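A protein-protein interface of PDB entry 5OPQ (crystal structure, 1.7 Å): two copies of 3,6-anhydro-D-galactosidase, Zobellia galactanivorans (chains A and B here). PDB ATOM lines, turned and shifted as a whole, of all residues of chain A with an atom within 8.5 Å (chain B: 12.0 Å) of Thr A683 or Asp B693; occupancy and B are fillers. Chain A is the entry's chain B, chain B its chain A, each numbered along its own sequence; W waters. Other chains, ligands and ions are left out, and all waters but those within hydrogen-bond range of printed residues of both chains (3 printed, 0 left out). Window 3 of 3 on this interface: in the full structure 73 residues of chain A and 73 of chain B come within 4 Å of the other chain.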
ATOM      1  N   LEU A 614     -23.152 -18.870  -4.486  1.00  0.00           N
ATOM      2  CA  LEU A 614     -24.005 -18.097  -5.249  1.00  0.00           C
ATOM      3  C   LEU A 614     -25.491 -18.365  -4.985  1.00  0.00           C
ATOM      4  O   LEU A 614     -26.248 -17.418  -4.741  1.00  0.00           O
ATOM      5  CB  LEU A 614     -23.776 -18.312  -6.769  1.00  0.00           C
ATOM      6  CG  LEU A 614     -24.717 -17.565  -7.722  1.00  0.00           C
ATOM      7  CD1 LEU A 614     -24.560 -16.022  -7.648  1.00  0.00           C
ATOM      8  CD2 LEU A 614     -24.460 -17.951  -9.190  1.00  0.00           C
ATOM      9  N   ILE A 651     -31.572 -10.956 -11.727  1.00  0.00           N
ATOM     10  CA  ILE A 651     -31.458 -10.787 -13.169  1.00  0.00           C
ATOM     11  C   ILE A 651     -30.369 -11.777 -13.540  1.00  0.00           C
ATOM     12  O   ILE A 651     -29.265 -11.811 -12.956  1.00  0.00           O
ATOM     13  CB  ILE A 651     -31.032  -9.396 -13.654  1.00  0.00           C
ATOM     14  CG1 ILE A 651     -32.146  -8.368 -13.281  1.00  0.00           C
ATOM     15  CG2 ILE A 651     -30.918  -9.360 -15.149  1.00  0.00           C
ATOM     16  CD1 ILE A 651     -31.751  -6.931 -13.569  1.00  0.00           C
ATOM     17  N   ILE A 665     -27.725  -1.194 -18.881  1.00  0.00           N
ATOM     18  CA  ILE A 665     -26.984  -2.087 -17.990  1.00  0.00           C
ATOM     19  C   ILE A 665     -26.678  -3.372 -18.784  1.00  0.00           C
ATOM     20  O   ILE A 665     -27.569  -3.827 -19.435  1.00  0.00           O
ATOM     21  CB  ILE A 665     -27.807  -2.532 -16.738  1.00  0.00           C
ATOM     22  CG1 ILE A 665     -28.109  -1.369 -15.772  1.00  0.00           C
ATOM     23  CG2 ILE A 665     -26.973  -3.481 -15.863  1.00  0.00           C
ATOM     24  CD1 ILE A 665     -26.889  -0.527 -15.515  1.00  0.00           C
ATOM     25  N   SER A 666     -25.462  -3.887 -18.660  1.00  0.00           N
ATOM     26  CA  SER A 666     -25.052  -5.116 -19.405  1.00  0.00           C
ATOM     27  C   SER A 666     -25.021  -6.269 -18.417  1.00  0.00           C
ATOM     28  O   SER A 666     -24.482  -6.194 -17.318  1.00  0.00           O
ATOM     29  CB  SER A 666     -23.744  -4.913 -20.169  1.00  0.00           C
ATOM     30  OG  SER A 666     -23.363  -6.139 -20.787  1.00  0.00           O
ATOM     31  N   ILE A 667     -25.575  -7.446 -18.819  1.00  0.00           N
ATOM     32  CA  ILE A 667     -25.499  -8.664 -18.011  1.00  0.00           C
ATOM     33  C   ILE A 667     -24.608  -9.639 -18.772  1.00  0.00           C
ATOM     34  O   ILE A 667     -24.899  -9.931 -19.929  1.00  0.00           O
ATOM     35  CB  ILE A 667     -26.871  -9.322 -17.838  1.00  0.00           C
ATOM     36  CG1 ILE A 667     -28.038  -8.329 -17.456  1.00  0.00           C
ATOM     37  CG2 ILE A 667     -26.732 -10.439 -16.828  1.00  0.00           C
ATOM     38  CD1 ILE A 667     -27.763  -7.657 -16.116  1.00  0.00           C
ATOM     39  N   PRO A 668     -23.487 -10.052 -18.182  1.00  0.00           N
ATOM     40  CA  PRO A 668     -22.563 -10.944 -18.906  1.00  0.00           C
ATOM     41  C   PRO A 668     -23.242 -12.261 -19.306  1.00  0.00           C
ATOM     42  O   PRO A 668     -24.197 -12.693 -18.682  1.00  0.00           O
ATOM     43  CB  PRO A 668     -21.509 -11.302 -17.930  1.00  0.00           C
ATOM     44  CG  PRO A 668     -21.550 -10.163 -16.888  1.00  0.00           C
ATOM     45  CD  PRO A 668     -22.986  -9.689 -16.841  1.00  0.00           C
ATOM     46  N   GLY A 671     -24.263 -14.825 -16.688  1.00  0.00           N
ATOM     47  CA  GLY A 671     -24.014 -13.858 -15.608  1.00  0.00           C
ATOM     48  C   GLY A 671     -25.278 -13.444 -14.875  1.00  0.00           C
ATOM     49  O   GLY A 671     -26.380 -13.781 -15.231  1.00  0.00           O
ATOM     50  N   TYR A 672     -25.074 -12.603 -13.863  1.00  0.00           N
ATOM     51  CA  TYR A 672     -26.178 -12.286 -12.925  1.00  0.00           C
ATOM     52  C   TYR A 672     -25.957 -10.895 -12.335  1.00  0.00           C
ATOM     53  O   TYR A 672     -24.839 -10.372 -12.314  1.00  0.00           O
ATOM     54  CB  TYR A 672     -26.294 -13.275 -11.841  1.00  0.00           C
ATOM     55  CG  TYR A 672     -25.113 -13.437 -10.952  1.00  0.00           C
ATOM     56  CD1 TYR A 672     -24.904 -12.582  -9.842  1.00  0.00           C
ATOM     57  CD2 TYR A 672     -24.130 -14.347 -11.234  1.00  0.00           C
ATOM     58  CE1 TYR A 672     -23.766 -12.691  -9.133  1.00  0.00           C
ATOM     59  CE2 TYR A 672     -22.984 -14.501 -10.451  1.00  0.00           C
ATOM     60  CZ  TYR A 672     -22.822 -13.647  -9.361  1.00  0.00           C
ATOM     61  OH  TYR A 672     -21.701 -13.695  -8.585  1.00  0.00           O
ATOM     62  N   ARG A 673     -27.091 -10.290 -12.012  1.00  0.00           N
ATOM     63  CA  ARG A 673     -27.084  -9.060 -11.147  1.00  0.00           C
ATOM     64  C   ARG A 673     -28.292  -9.219 -10.206  1.00  0.00           C
ATOM     65  O   ARG A 673     -29.450  -9.269 -10.674  1.00  0.00           O
ATOM     66  CB  ARG A 673     -27.254  -7.924 -12.065  1.00  0.00           C
ATOM     67  CG  ARG A 673     -27.448  -6.598 -11.401  1.00  0.00           C
ATOM     68  CD  ARG A 673     -27.783  -5.641 -12.536  1.00  0.00           C
ATOM     69  NE  ARG A 673     -26.663  -4.792 -12.682  1.00  0.00           N
ATOM     70  CZ  ARG A 673     -26.460  -3.748 -11.916  1.00  0.00           C
ATOM     71  NH1 ARG A 673     -25.361  -3.065 -12.091  1.00  0.00           N
ATOM     72  NH2 ARG A 673     -27.364  -3.387 -11.004  1.00  0.00           N
ATOM     73  N   ILE A 674     -27.968  -9.253  -8.927  1.00  0.00           N
ATOM     74  CA  ILE A 674     -28.918  -9.592  -7.908  1.00  0.00           C
ATOM     75  C   ILE A 674     -28.907  -8.458  -6.869  1.00  0.00           C
ATOM     76  O   ILE A 674     -27.878  -8.107  -6.435  1.00  0.00           O
ATOM     77  CB  ILE A 674     -28.523 -10.823  -7.225  1.00  0.00           C
ATOM     78  CG1 ILE A 674     -28.518 -12.014  -8.273  1.00  0.00           C
ATOM     79  CG2 ILE A 674     -29.467 -11.165  -6.068  1.00  0.00           C
ATOM     80  CD1 ILE A 674     -27.963 -13.267  -7.791  1.00  0.00           C
ATOM     81  N   GLN A 675     -30.072  -7.942  -6.621  1.00  0.00           N
ATOM     82  CA  GLN A 675     -30.310  -6.915  -5.524  1.00  0.00           C
ATOM     83  C   GLN A 675     -30.904  -7.669  -4.344  1.00  0.00           C
ATOM     84  O   GLN A 675     -32.029  -8.204  -4.439  1.00  0.00           O
ATOM     85  CB  GLN A 675     -31.286  -5.844  -6.078  1.00  0.00           C
ATOM     86  N   SER A 680     -27.839  -4.515  -0.937  1.00  0.00           N
ATOM     87  CA  SER A 680     -26.560  -4.772  -1.551  1.00  0.00           C
ATOM     88  C   SER A 680     -26.777  -5.403  -2.985  1.00  0.00           C
ATOM     89  O   SER A 680     -27.843  -5.950  -3.275  1.00  0.00           O
ATOM     90  CB  SER A 680     -25.743  -5.670  -0.672  1.00  0.00           C
ATOM     91  OG  SER A 680     -26.249  -6.958  -0.535  1.00  0.00           O
ATOM     92  N   LEU A 681     -25.760  -5.288  -3.826  1.00  0.00           N
ATOM     93  CA  LEU A 681     -25.814  -5.747  -5.224  1.00  0.00           C
ATOM     94  C   LEU A 681     -24.710  -6.780  -5.409  1.00  0.00           C
ATOM     95  O   LEU A 681     -23.587  -6.551  -4.993  1.00  0.00           O
ATOM     96  CB  LEU A 681     -25.575  -4.546  -6.090  1.00  0.00           C
ATOM     97  CG  LEU A 681     -25.803  -4.696  -7.570  1.00  0.00           C
ATOM     98  CD1 LEU A 681     -27.338  -4.744  -7.838  1.00  0.00           C
ATOM     99  CD2 LEU A 681     -25.106  -3.564  -8.300  1.00  0.00           C
ATOM    100  N   LYS A 682     -25.044  -7.946  -5.988  1.00  0.00           N
ATOM    101  CA  LYS A 682     -24.099  -8.992  -6.291  1.00  0.00           C
ATOM    102  C   LYS A 682     -24.110  -9.069  -7.831  1.00  0.00           C
ATOM    103  O   LYS A 682     -25.160  -9.209  -8.462  1.00  0.00           O
ATOM    104  CB  LYS A 682     -24.605 -10.310  -5.695  1.00  0.00           C
ATOM    105  CG  LYS A 682     -24.632 -10.447  -4.180  1.00  0.00           C
ATOM    106  CD  LYS A 682     -24.897 -11.916  -3.848  1.00  0.00           C
ATOM    107  CE  LYS A 682     -24.834 -12.322  -2.370  1.00  0.00           C
ATOM    108  NZ  LYS A 682     -26.047 -13.161  -2.117  1.00  0.00           N
ATOM    109  N   THR A 683     -22.938  -8.959  -8.442  1.00  0.00           N
ATOM    110  CA  THR A 683     -22.823  -9.106  -9.907  1.00  0.00           C
ATOM    111  C   THR A 683     -21.709 -10.156 -10.103  1.00  0.00           C
ATOM    112  O   THR A 683     -20.798 -10.328  -9.265  1.00  0.00           O
ATOM    113  CB  THR A 683     -22.490  -7.820 -10.600  1.00  0.00           C
ATOM    114  OG1 THR A 683     -21.293  -7.256 -10.064  1.00  0.00           O
ATOM    115  CG2 THR A 683     -23.665  -6.841 -10.449  1.00  0.00           C
ATOM    116  N   GLY A 684     -21.762 -10.834 -11.260  1.00  0.00           N
ATOM    117  CA  GLY A 684     -20.785 -11.887 -11.436  1.00  0.00           C
ATOM    118  C   GLY A 684     -21.175 -12.751 -12.659  1.00  0.00           C
ATOM    119  O   GLY A 684     -22.189 -12.432 -13.334  1.00  0.00           O
ATOM    120  N   HIS A 685     -20.295 -13.715 -12.942  1.00  0.00           N
ATOM    121  CA  HIS A 685     -20.571 -14.648 -14.123  1.00  0.00           C
ATOM    122  C   HIS A 685     -19.773 -15.861 -13.994  1.00  0.00           C
ATOM    123  O   HIS A 685     -18.836 -15.970 -13.194  1.00  0.00           O
ATOM    124  CB  HIS A 685     -20.263 -13.957 -15.453  1.00  0.00           C
ATOM    125  CG  HIS A 685     -18.808 -13.718 -15.635  1.00  0.00           C
ATOM    126  ND1 HIS A 685     -18.147 -12.629 -15.084  1.00  0.00           N
ATOM    127  CD2 HIS A 685     -17.873 -14.456 -16.265  1.00  0.00           C
ATOM    128  CE1 HIS A 685     -16.863 -12.723 -15.377  1.00  0.00           C
ATOM    129  NE2 HIS A 685     -16.682 -13.798 -16.118  1.00  0.00           N
ATOM    130  N   PHE A 686     -20.200 -16.962 -14.694  1.00  0.00           N
ATOM    131  CA  PHE A 686     -19.453 -18.158 -14.765  1.00  0.00           C
ATOM    132  C   PHE A 686     -18.539 -18.113 -15.968  1.00  0.00           C
ATOM    133  O   PHE A 686     -18.839 -17.512 -16.987  1.00  0.00           O
ATOM    134  CB  PHE A 686     -20.385 -19.398 -14.941  1.00  0.00           C
ATOM    135  CG  PHE A 686     -21.238 -19.716 -13.748  1.00  0.00           C
ATOM    136  CD1 PHE A 686     -20.736 -20.542 -12.746  1.00  0.00           C
ATOM    137  CD2 PHE A 686     -22.547 -19.212 -13.619  1.00  0.00           C
ATOM    138  CE1 PHE A 686     -21.511 -20.915 -11.700  1.00  0.00           C
ATOM    139  CE2 PHE A 686     -23.330 -19.614 -12.565  1.00  0.00           C
ATOM    140  CZ  PHE A 686     -22.781 -20.392 -11.565  1.00  0.00           C
ATOM    141  N   GLN A 687     -17.399 -18.778 -15.799  1.00  0.00           N
ATOM    142  CA  GLN A 687     -16.421 -18.901 -16.911  1.00  0.00           C
ATOM    143  C   GLN A 687     -16.008 -20.312 -17.039  1.00  0.00           C
ATOM    144  O   GLN A 687     -15.746 -21.014 -16.079  1.00  0.00           O
ATOM    145  CB  GLN A 687     -15.144 -18.055 -16.651  1.00  0.00           C
ATOM    146  CG  GLN A 687     -15.332 -16.627 -17.056  1.00  0.00           C
ATOM    147  CD  GLN A 687     -13.997 -15.817 -17.123  1.00  0.00           C
ATOM    148  OE1 GLN A 687     -12.978 -16.339 -17.585  1.00  0.00           O
ATOM    149  NE2 GLN A 687     -14.016 -14.532 -16.657  1.00  0.00           N
ATOM    150  N   SER B 689     -15.550 -21.883 -13.411  1.00  0.00           N
ATOM    151  CA  SER B 689     -15.356 -21.063 -12.212  1.00  0.00           C
ATOM    152  C   SER B 689     -16.439 -20.051 -12.091  1.00  0.00           C
ATOM    153  O   SER B 689     -17.037 -19.625 -13.052  1.00  0.00           O
ATOM    154  CB  SER B 689     -13.939 -20.529 -12.286  1.00  0.00           C
ATOM    155  OG  SER B 689     -13.670 -19.767 -13.336  1.00  0.00           O
ATOM    156  N   LEU B 690     -16.612 -19.500 -10.881  1.00  0.00           N
ATOM    157  CA  LEU B 690     -17.571 -18.458 -10.628  1.00  0.00           C
ATOM    158  C   LEU B 690     -16.759 -17.221 -10.322  1.00  0.00           C
ATOM    159  O   LEU B 690     -15.976 -17.269  -9.369  1.00  0.00           O
ATOM    160  CB  LEU B 690     -18.413 -18.870  -9.431  1.00  0.00           C
ATOM    161  CG  LEU B 690     -19.432 -17.891  -8.898  1.00  0.00           C
ATOM    162  CD1 LEU B 690     -20.339 -17.397  -9.988  1.00  0.00           C
ATOM    163  CD2 LEU B 690     -20.173 -18.589  -7.761  1.00  0.00           C
ATOM    164  N   HIS B 691     -17.009 -16.153 -11.064  1.00  0.00           N
ATOM    165  CA  HIS B 691     -16.403 -14.877 -10.805  1.00  0.00           C
ATOM    166  C   HIS B 691     -17.418 -13.972 -10.124  1.00  0.00           C
ATOM    167  O   HIS B 691     -18.280 -13.451 -10.823  1.00  0.00           O
ATOM    168  CB  HIS B 691     -15.939 -14.247 -12.094  1.00  0.00           C
ATOM    169  CG  HIS B 691     -14.908 -15.049 -12.713  1.00  0.00           C
ATOM    170  ND1 HIS B 691     -13.573 -14.754 -12.521  1.00  0.00           N
ATOM    171  CD2 HIS B 691     -14.956 -16.252 -13.333  1.00  0.00           C
ATOM    172  CE1 HIS B 691     -12.848 -15.714 -13.084  1.00  0.00           C
ATOM    173  NE2 HIS B 691     -13.650 -16.641 -13.569  1.00  0.00           N
ATOM    174  N   MET B 692     -17.278 -13.782  -8.790  1.00  0.00           N
ATOM    175  CA  MET B 692     -18.157 -12.874  -8.022  1.00  0.00           C
ATOM    176  C   MET B 692     -17.452 -11.547  -7.936  1.00  0.00           C
ATOM    177  O   MET B 692     -16.353 -11.548  -7.477  1.00  0.00           O
ATOM    178  CB  MET B 692     -18.454 -13.476  -6.642  1.00  0.00           C
ATOM    179  CG  MET B 692     -19.141 -14.817  -6.718  1.00  0.00           C
ATOM    180  SD  MET B 692     -19.825 -15.438  -5.144  1.00  0.00           S
ATOM    181  CE  MET B 692     -18.215 -16.063  -4.608  1.00  0.00           C
ATOM    182  N   ASP B 693     -18.045 -10.454  -8.433  1.00  0.00           N
ATOM    183  CA  ASP B 693     -17.355  -9.151  -8.500  1.00  0.00           C
ATOM    184  C   ASP B 693     -17.303  -8.580  -7.084  1.00  0.00           C
ATOM    185  O   ASP B 693     -16.437  -7.755  -6.847  1.00  0.00           O
ATOM    186  CB  ASP B 693     -18.059  -8.173  -9.448  1.00  0.00           C
ATOM    187  CG  ASP B 693     -18.251  -8.758 -10.880  1.00  0.00           C
ATOM    188  OD1 ASP B 693     -17.463  -9.629 -11.266  1.00  0.00           O
ATOM    189  OD2 ASP B 693     -19.217  -8.335 -11.540  1.00  0.00           O
ATOM    190  OXT ASP B 693     -18.073  -8.970  -6.189  1.00  0.00           O
HETATM  191  O   HOH W   1     -12.764 -21.315 -15.266  1.00  0.00           O
HETATM  192  O   HOH W   2     -20.537  -8.761  -6.556  1.00  0.00           O
HETATM  193  O   HOH W   3     -19.201 -10.119 -14.128  1.00  0.00           O
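N of Ser B689 is in hydrogen-bond range of O of Gln A687, at 2.8 Å.
O of His A685 lies within hydrogen-bond range of N of His B691 (2.8 Å).
OD2 of Asp B693 is in hydrogen-bond range of OG1 of Thr A683, 2.8 Å away.
The side-chain hydroxyl (OG) of Ser B689 sits at hydrogen-bond distance from a ring nitrogen (NE2) of His B691, at 3.1 Å.
The backbone NH (N) of Tyr A672 sits at hydrogen-bond distance from the backbone carbonyl oxygen (O) of Gly A684, 2.9 Å away.
NE2 of Gln A687 lies within hydrogen-bond range of NE2 of His A685.
CB of Leu A614 touches CD2 of Leu B690, at 3.7 Å.
Leu B690 touches Tyr A672 (CD1 to CE2, 3.9 Å).
Met B692 touches Tyr A672.
Met B692 touches Thr A683 (C to O, 3.8 Å).
Gly A684 touches His B691.
Asp B693 touches Gly A684.
C of Leu B690 touches O of His A685, at 3.8 Å.
Phe A686 touches Ser B689 (CA to O, 3.3 Å).
His B691 touches Gln A687 (NE2 to CD, 3.7 Å).
Thr A683 touches just these residues of chain B: Met B692 and Asp B693.
Asp B693 touches two residues of chain A.
Of chain B, only Leu B690 (3.9 Å) and Met B692 (3.4 Å) come within 4 Å of Tyr A672.
No residue of chain B comes within 4 Å of Arg A673.
No residue of chain B comes within 4 Å of Leu A681.
His A685 touches two residues of chain B.
Printed residues of chain A within 4 Å of Leu B690: Leu A614 (3.7 Å), Tyr A672 (3.9 Å) and His A685 (3.8 Å).
Of the printed residues of chain A, His B691 touches Gly A684, His A685 and Gln A687.
Of the printed residues of chain B, Gln A687 touches Ser B689 (2.8 Å) and His B691 (3.7 Å).
Printed residues of chain B within 4 Å of Phe A686: Ser B689.
Ile A651 touches none of the printed residues of chain B.
The nearest printed residue of chain A that does not touch Met B692 is Gly A684 (4.4 Å).
Of the 19 printed residues of chain A, 7 touch a printed residue of chain B.
Of the 5 printed residues of chain B, 5 touch a printed residue of chain A.
Hydrophobic or aromatic side chains of chain B that line the printed part of chain A: Leu B690, His B691 and Met B692.
No position is printed for both chains.
Of the 12 pairs that touch across the chains among the printed residues, none has its exchanged pair printed and touching as well.
Water W2 lies within hydrogen-bond range of OXT of Asp B693 (2.5 Å) and N of Thr A683 (3.1 Å).
Water W1 lies within hydrogen-bond range of OG of Ser B689 and O of Gln A687.
Water W3 bridges ND1 of His A685 (2.9 Å) and OD2 of Asp B693 (3.1 Å).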
